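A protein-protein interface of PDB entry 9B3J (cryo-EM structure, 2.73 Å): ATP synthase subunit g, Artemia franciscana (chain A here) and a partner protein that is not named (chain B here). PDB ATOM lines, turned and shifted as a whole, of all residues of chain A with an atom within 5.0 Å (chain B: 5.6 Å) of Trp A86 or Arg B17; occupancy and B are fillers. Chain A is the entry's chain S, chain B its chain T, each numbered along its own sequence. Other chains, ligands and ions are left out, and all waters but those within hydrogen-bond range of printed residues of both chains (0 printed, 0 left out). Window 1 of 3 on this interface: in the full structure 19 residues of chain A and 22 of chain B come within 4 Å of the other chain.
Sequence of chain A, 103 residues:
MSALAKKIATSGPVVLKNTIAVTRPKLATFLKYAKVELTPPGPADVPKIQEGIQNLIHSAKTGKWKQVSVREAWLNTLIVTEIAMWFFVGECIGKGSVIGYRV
The side-chain carboxylate of Glu A82 is in salt-bridge range of the guanidinium group of Arg B17, 3.0 Å away.
The backbone carbonyl oxygen (O) of Leu A38 sits close to the side-chain hydroxyl (OH) of Tyr B18 (2.4 Å).
NH1 of Arg B17 lies close to O of Ile B13.
Ile A83 touches Gly B16 (CG2 to O, 3.7 Å).
Ile A83 touches Ala B20.
Trp A86 touches Arg B17.
Trp A86 touches Leu B21 (O to CD1, 3.4 Å).
Ala B20 touches Phe A87 (O to CD1, 3.3 Å).
CA of Gly A90 touches CD1 of Leu B21, 3.7 Å away.
Printed residues of chain B within 4 Å of Ile A83: Gly B16 and Ala B20.
Trp A86 touches two residues of chain B.
Of the printed residues of chain B, Gly A90 touches Leu B21.
Arg B17 touches just these residues of chain A: Glu A82 (3.0 Å) and Trp A86 (3.5 Å).
Val B22 touches none of the printed residues of chain A.
The nearest residue of chain A that does not touch Arg B17 is Ile A83 (4.1 Å).
Of the 10 printed residues of chain A, 6 touch a printed residue of chain B.
Hydrophobic or aromatic side chains of chain A that line the printed part of chain B: Ile A83, Trp A86 and Phe A87.
Of the 12 printed residues of chain B, 5 touch a printed residue of chain A.
Hydrophobic or aromatic side chains of chain B within 4 Å of the printed part of chain A: Tyr B18, Ala B20 and Leu B21.
Along chain B the printed residues that touch a printed residue of chain A span positions 16 to 21.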
ATOM      1  N   LEU A  38     -16.698 -19.370  19.221  1.00  0.00           N
ATOM      2  CA  LEU A  38     -16.622 -19.971  20.554  1.00  0.00           C
ATOM      3  C   LEU A  38     -15.387 -20.847  20.721  1.00  0.00           C
ATOM      4  O   LEU A  38     -15.427 -21.873  21.402  1.00  0.00           O
ATOM      5  CB  LEU A  38     -17.885 -20.769  20.857  1.00  0.00           C
ATOM      6  CG  LEU A  38     -19.207 -20.021  20.713  1.00  0.00           C
ATOM      7  CD1 LEU A  38     -20.352 -20.875  21.213  1.00  0.00           C
ATOM      8  CD2 LEU A  38     -19.156 -18.706  21.460  1.00  0.00           C
ATOM      9  N   GLU A  82     -21.779 -11.440  30.191  1.00  0.00           N
ATOM     10  CA  GLU A  82     -21.644 -12.674  29.414  1.00  0.00           C
ATOM     11  C   GLU A  82     -20.429 -13.485  29.851  1.00  0.00           C
ATOM     12  O   GLU A  82     -20.494 -14.719  29.926  1.00  0.00           O
ATOM     13  CB  GLU A  82     -21.572 -12.359  27.922  1.00  0.00           C
ATOM     14  CG  GLU A  82     -21.371 -13.533  27.029  1.00  0.00           C
ATOM     15  CD  GLU A  82     -21.265 -13.130  25.578  1.00  0.00           C
ATOM     16  OE1 GLU A  82     -21.976 -12.190  25.164  1.00  0.00           O
ATOM     17  OE2 GLU A  82     -20.464 -13.750  24.851  1.00  0.00           O
ATOM     18  N   ILE A  83     -19.316 -12.807  30.133  1.00  0.00           N
ATOM     19  CA  ILE A  83     -18.125 -13.505  30.639  1.00  0.00           C
ATOM     20  C   ILE A  83     -18.418 -14.164  31.987  1.00  0.00           C
ATOM     21  O   ILE A  83     -18.058 -15.326  32.229  1.00  0.00           O
ATOM     22  CB  ILE A  83     -16.936 -12.532  30.727  1.00  0.00           C
ATOM     23  CG1 ILE A  83     -16.484 -12.127  29.329  1.00  0.00           C
ATOM     24  CG2 ILE A  83     -15.790 -13.133  31.505  1.00  0.00           C
ATOM     25  CD1 ILE A  83     -15.339 -11.163  29.334  1.00  0.00           C
ATOM     26  N   ALA A  84     -19.100 -13.441  32.871  1.00  0.00           N
ATOM     27  CA  ALA A  84     -19.464 -14.007  34.169  1.00  0.00           C
ATOM     28  C   ALA A  84     -20.463 -15.154  34.030  1.00  0.00           C
ATOM     29  O   ALA A  84     -20.441 -16.106  34.823  1.00  0.00           O
ATOM     30  CB  ALA A  84     -20.027 -12.921  35.079  1.00  0.00           C
ATOM     31  N   MET A  85     -21.330 -15.101  33.022  1.00  0.00           N
ATOM     32  CA  MET A  85     -22.238 -16.218  32.796  1.00  0.00           C
ATOM     33  C   MET A  85     -21.509 -17.428  32.223  1.00  0.00           C
ATOM     34  O   MET A  85     -21.901 -18.567  32.494  1.00  0.00           O
ATOM     35  CB  MET A  85     -23.383 -15.781  31.890  1.00  0.00           C
ATOM     36  CG  MET A  85     -24.426 -14.989  32.636  1.00  0.00           C
ATOM     37  SD  MET A  85     -25.514 -14.058  31.559  1.00  0.00           S
ATOM     38  CE  MET A  85     -26.509 -13.212  32.784  1.00  0.00           C
ATOM     39  N   TRP A  86     -20.448 -17.205  31.442  1.00  0.00           N
ATOM     40  CA  TRP A  86     -19.588 -18.313  31.035  1.00  0.00           C
ATOM     41  C   TRP A  86     -18.871 -18.921  32.229  1.00  0.00           C
ATOM     42  O   TRP A  86     -18.632 -20.132  32.259  1.00  0.00           O
ATOM     43  CB  TRP A  86     -18.570 -17.852  29.995  1.00  0.00           C
ATOM     44  CG  TRP A  86     -19.036 -18.026  28.590  1.00  0.00           C
ATOM     45  CD1 TRP A  86     -19.912 -17.233  27.917  1.00  0.00           C
ATOM     46  CD2 TRP A  86     -18.649 -19.058  27.680  1.00  0.00           C
ATOM     47  NE1 TRP A  86     -20.099 -17.707  26.644  1.00  0.00           N
ATOM     48  CE2 TRP A  86     -19.332 -18.828  26.474  1.00  0.00           C
ATOM     49  CE3 TRP A  86     -17.790 -20.150  27.766  1.00  0.00           C
ATOM     50  CZ2 TRP A  86     -19.185 -19.651  25.366  1.00  0.00           C
ATOM     51  CZ3 TRP A  86     -17.646 -20.967  26.665  1.00  0.00           C
ATOM     52  CH2 TRP A  86     -18.340 -20.713  25.481  1.00  0.00           C
ATOM     53  N   PHE A  87     -18.525 -18.090  33.213  1.00  0.00           N
ATOM     54  CA  PHE A  87     -17.940 -18.598  34.453  1.00  0.00           C
ATOM     55  C   PHE A  87     -18.916 -19.497  35.202  1.00  0.00           C
ATOM     56  O   PHE A  87     -18.525 -20.533  35.750  1.00  0.00           O
ATOM     57  CB  PHE A  87     -17.502 -17.429  35.333  1.00  0.00           C
ATOM     58  CG  PHE A  87     -17.381 -17.766  36.788  1.00  0.00           C
ATOM     59  CD1 PHE A  87     -16.271 -18.427  37.265  1.00  0.00           C
ATOM     60  CD2 PHE A  87     -18.362 -17.386  37.687  1.00  0.00           C
ATOM     61  CE1 PHE A  87     -16.150 -18.729  38.605  1.00  0.00           C
ATOM     62  CE2 PHE A  87     -18.248 -17.689  39.026  1.00  0.00           C
ATOM     63  CZ  PHE A  87     -17.140 -18.361  39.484  1.00  0.00           C
ATOM     64  N   PHE A  88     -20.190 -19.111  35.244  1.00  0.00           N
ATOM     65  CA  PHE A  88     -21.173 -19.952  35.929  1.00  0.00           C
ATOM     66  C   PHE A  88     -21.531 -21.195  35.124  1.00  0.00           C
ATOM     67  O   PHE A  88     -21.897 -22.223  35.706  1.00  0.00           O
ATOM     68  CB  PHE A  88     -22.429 -19.153  36.245  1.00  0.00           C
ATOM     69  CG  PHE A  88     -22.311 -18.327  37.481  1.00  0.00           C
ATOM     70  CD1 PHE A  88     -22.479 -18.903  38.723  1.00  0.00           C
ATOM     71  CD2 PHE A  88     -22.027 -16.977  37.404  1.00  0.00           C
ATOM     72  CE1 PHE A  88     -22.370 -18.147  39.867  1.00  0.00           C
ATOM     73  CE2 PHE A  88     -21.915 -16.218  38.540  1.00  0.00           C
ATOM     74  CZ  PHE A  88     -22.088 -16.802  39.774  1.00  0.00           C
ATOM     75  N   VAL A  89     -21.445 -21.125  33.796  1.00  0.00           N
ATOM     76  CA  VAL A  89     -21.580 -22.328  32.981  1.00  0.00           C
ATOM     77  C   VAL A  89     -20.442 -23.291  33.281  1.00  0.00           C
ATOM     78  O   VAL A  89     -20.657 -24.499  33.443  1.00  0.00           O
ATOM     79  CB  VAL A  89     -21.639 -21.954  31.489  1.00  0.00           C
ATOM     80  CG1 VAL A  89     -21.349 -23.153  30.610  1.00  0.00           C
ATOM     81  CG2 VAL A  89     -22.998 -21.382  31.153  1.00  0.00           C
ATOM     82  N   GLY A  90     -19.218 -22.769  33.379  1.00  0.00           N
ATOM     83  CA  GLY A  90     -18.093 -23.597  33.775  1.00  0.00           C
ATOM     84  C   GLY A  90     -18.229 -24.150  35.176  1.00  0.00           C
ATOM     85  O   GLY A  90     -17.779 -25.260  35.457  1.00  0.00           O
ATOM     86  N   VAL B   9     -14.182 -12.505  17.553  1.00  0.00           N
ATOM     87  CA  VAL B   9     -14.279 -11.771  18.802  1.00  0.00           C
ATOM     88  C   VAL B   9     -12.916 -11.189  19.162  1.00  0.00           C
ATOM     89  O   VAL B   9     -11.872 -11.608  18.650  1.00  0.00           O
ATOM     90  CB  VAL B   9     -14.814 -12.690  19.912  1.00  0.00           C
ATOM     91  CG1 VAL B   9     -15.580 -11.902  20.951  1.00  0.00           C
ATOM     92  CG2 VAL B   9     -15.708 -13.757  19.318  1.00  0.00           C
ATOM     93  N   LEU B  12      -8.983 -10.333  23.886  1.00  0.00           N
ATOM     94  CA  LEU B  12      -9.157 -10.135  25.322  1.00  0.00           C
ATOM     95  C   LEU B  12     -10.477 -10.723  25.805  1.00  0.00           C
ATOM     96  O   LEU B  12     -10.541 -11.320  26.887  1.00  0.00           O
ATOM     97  CB  LEU B  12      -9.078  -8.643  25.655  1.00  0.00           C
ATOM     98  CG  LEU B  12      -9.506  -8.206  27.057  1.00  0.00           C
ATOM     99  CD1 LEU B  12      -8.642  -8.857  28.122  1.00  0.00           C
ATOM    100  CD2 LEU B  12      -9.467  -6.692  27.191  1.00  0.00           C
ATOM    101  N   ILE B  13     -11.539 -10.568  25.011  1.00  0.00           N
ATOM    102  CA  ILE B  13     -12.836 -11.130  25.374  1.00  0.00           C
ATOM    103  C   ILE B  13     -12.767 -12.649  25.408  1.00  0.00           C
ATOM    104  O   ILE B  13     -13.256 -13.285  26.349  1.00  0.00           O
ATOM    105  CB  ILE B  13     -13.921 -10.633  24.404  1.00  0.00           C
ATOM    106  CG1 ILE B  13     -14.053  -9.119  24.487  1.00  0.00           C
ATOM    107  CG2 ILE B  13     -15.254 -11.267  24.722  1.00  0.00           C
ATOM    108  CD1 ILE B  13     -15.053  -8.559  23.517  1.00  0.00           C
ATOM    109  N   ARG B  14     -12.143 -13.253  24.397  1.00  0.00           N
ATOM    110  CA  ARG B  14     -12.037 -14.708  24.359  1.00  0.00           C
ATOM    111  C   ARG B  14     -11.163 -15.232  25.492  1.00  0.00           C
ATOM    112  O   ARG B  14     -11.482 -16.261  26.106  1.00  0.00           O
ATOM    113  CB  ARG B  14     -11.485 -15.161  23.009  1.00  0.00           C
ATOM    114  CG  ARG B  14     -12.529 -15.393  21.931  1.00  0.00           C
ATOM    115  CD  ARG B  14     -11.867 -15.957  20.690  1.00  0.00           C
ATOM    116  NE  ARG B  14     -12.770 -16.043  19.550  1.00  0.00           N
ATOM    117  CZ  ARG B  14     -12.391 -16.400  18.331  1.00  0.00           C
ATOM    118  NH1 ARG B  14     -11.140 -16.731  18.066  1.00  0.00           N
ATOM    119  NH2 ARG B  14     -13.289 -16.418  17.351  1.00  0.00           N
ATOM    120  N   ALA B  15     -10.062 -14.537  25.785  1.00  0.00           N
ATOM    121  CA  ALA B  15      -9.169 -14.980  26.848  1.00  0.00           C
ATOM    122  C   ALA B  15      -9.841 -14.881  28.206  1.00  0.00           C
ATOM    123  O   ALA B  15      -9.737 -15.803  29.019  1.00  0.00           O
ATOM    124  CB  ALA B  15      -7.878 -14.165  26.828  1.00  0.00           C
ATOM    125  N   GLY B  16     -10.551 -13.780  28.461  1.00  0.00           N
ATOM    126  CA  GLY B  16     -11.262 -13.645  29.722  1.00  0.00           C
ATOM    127  C   GLY B  16     -12.415 -14.618  29.852  1.00  0.00           C
ATOM    128  O   GLY B  16     -12.688 -15.123  30.942  1.00  0.00           O
ATOM    129  N   ARG B  17     -13.094 -14.910  28.741  1.00  0.00           N
ATOM    130  CA  ARG B  17     -14.224 -15.832  28.771  1.00  0.00           C
ATOM    131  C   ARG B  17     -13.773 -17.250  29.078  1.00  0.00           C
ATOM    132  O   ARG B  17     -14.354 -17.926  29.937  1.00  0.00           O
ATOM    133  CB  ARG B  17     -14.954 -15.784  27.435  1.00  0.00           C
ATOM    134  CG  ARG B  17     -15.984 -16.865  27.260  1.00  0.00           C
ATOM    135  CD  ARG B  17     -16.464 -16.931  25.821  1.00  0.00           C
ATOM    136  NE  ARG B  17     -17.227 -15.753  25.424  1.00  0.00           N
ATOM    137  CZ  ARG B  17     -16.751 -14.766  24.678  1.00  0.00           C
ATOM    138  NH1 ARG B  17     -15.504 -14.769  24.244  1.00  0.00           N
ATOM    139  NH2 ARG B  17     -17.549 -13.751  24.361  1.00  0.00           N
ATOM    140  N   TYR B  18     -12.727 -17.720  28.397  1.00  0.00           N
ATOM    141  CA  TYR B  18     -12.241 -19.065  28.676  1.00  0.00           C
ATOM    142  C   TYR B  18     -11.468 -19.137  29.983  1.00  0.00           C
ATOM    143  O   TYR B  18     -11.458 -20.192  30.629  1.00  0.00           O
ATOM    144  CB  TYR B  18     -11.387 -19.566  27.521  1.00  0.00           C
ATOM    145  CG  TYR B  18     -12.211 -20.245  26.464  1.00  0.00           C
ATOM    146  CD1 TYR B  18     -12.674 -21.538  26.648  1.00  0.00           C
ATOM    147  CD2 TYR B  18     -12.543 -19.592  25.292  1.00  0.00           C
ATOM    148  CE1 TYR B  18     -13.435 -22.167  25.690  1.00  0.00           C
ATOM    149  CE2 TYR B  18     -13.304 -20.211  24.328  1.00  0.00           C
ATOM    150  CZ  TYR B  18     -13.746 -21.499  24.532  1.00  0.00           C
ATOM    151  OH  TYR B  18     -14.505 -22.119  23.568  1.00  0.00           O
ATOM    152  N   GLY B  19     -10.838 -18.037  30.403  1.00  0.00           N
ATOM    153  CA  GLY B  19     -10.257 -17.997  31.730  1.00  0.00           C
ATOM    154  C   GLY B  19     -11.309 -18.117  32.814  1.00  0.00           C
ATOM    155  O   GLY B  19     -11.124 -18.846  33.794  1.00  0.00           O
ATOM    156  N   ALA B  20     -12.439 -17.430  32.636  1.00  0.00           N
ATOM    157  CA  ALA B  20     -13.554 -17.563  33.562  1.00  0.00           C
ATOM    158  C   ALA B  20     -14.167 -18.953  33.506  1.00  0.00           C
ATOM    159  O   ALA B  20     -14.640 -19.455  34.526  1.00  0.00           O
ATOM    160  CB  ALA B  20     -14.613 -16.507  33.262  1.00  0.00           C
ATOM    161  N   LEU B  21     -14.163 -19.586  32.332  1.00  0.00           N
ATOM    162  CA  LEU B  21     -14.659 -20.956  32.228  1.00  0.00           C
ATOM    163  C   LEU B  21     -13.787 -21.925  33.017  1.00  0.00           C
ATOM    164  O   LEU B  21     -14.300 -22.797  33.735  1.00  0.00           O
ATOM    165  CB  LEU B  21     -14.715 -21.372  30.763  1.00  0.00           C
ATOM    166  CG  LEU B  21     -15.416 -22.688  30.466  1.00  0.00           C
ATOM    167  CD1 LEU B  21     -16.900 -22.474  30.513  1.00  0.00           C
ATOM    168  CD2 LEU B  21     -14.998 -23.196  29.110  1.00  0.00           C
ATOM    169  N   VAL B  22     -12.465 -21.778  32.901  1.00  0.00           N
ATOM    170  CA  VAL B  22     -11.541 -22.648  33.626  1.00  0.00           C
ATOM    171  C   VAL B  22     -11.647 -22.416  35.129  1.00  0.00           C
ATOM    172  O   VAL B  22     -11.702 -23.374  35.923  1.00  0.00           O
ATOM    173  CB  VAL B  22     -10.107 -22.425  33.115  1.00  0.00           C
ATOM    174  CG1 VAL B  22      -9.107 -23.146  33.998  1.00  0.00           C
ATOM    175  CG2 VAL B  22      -9.984 -22.902  31.681  1.00  0.00           C
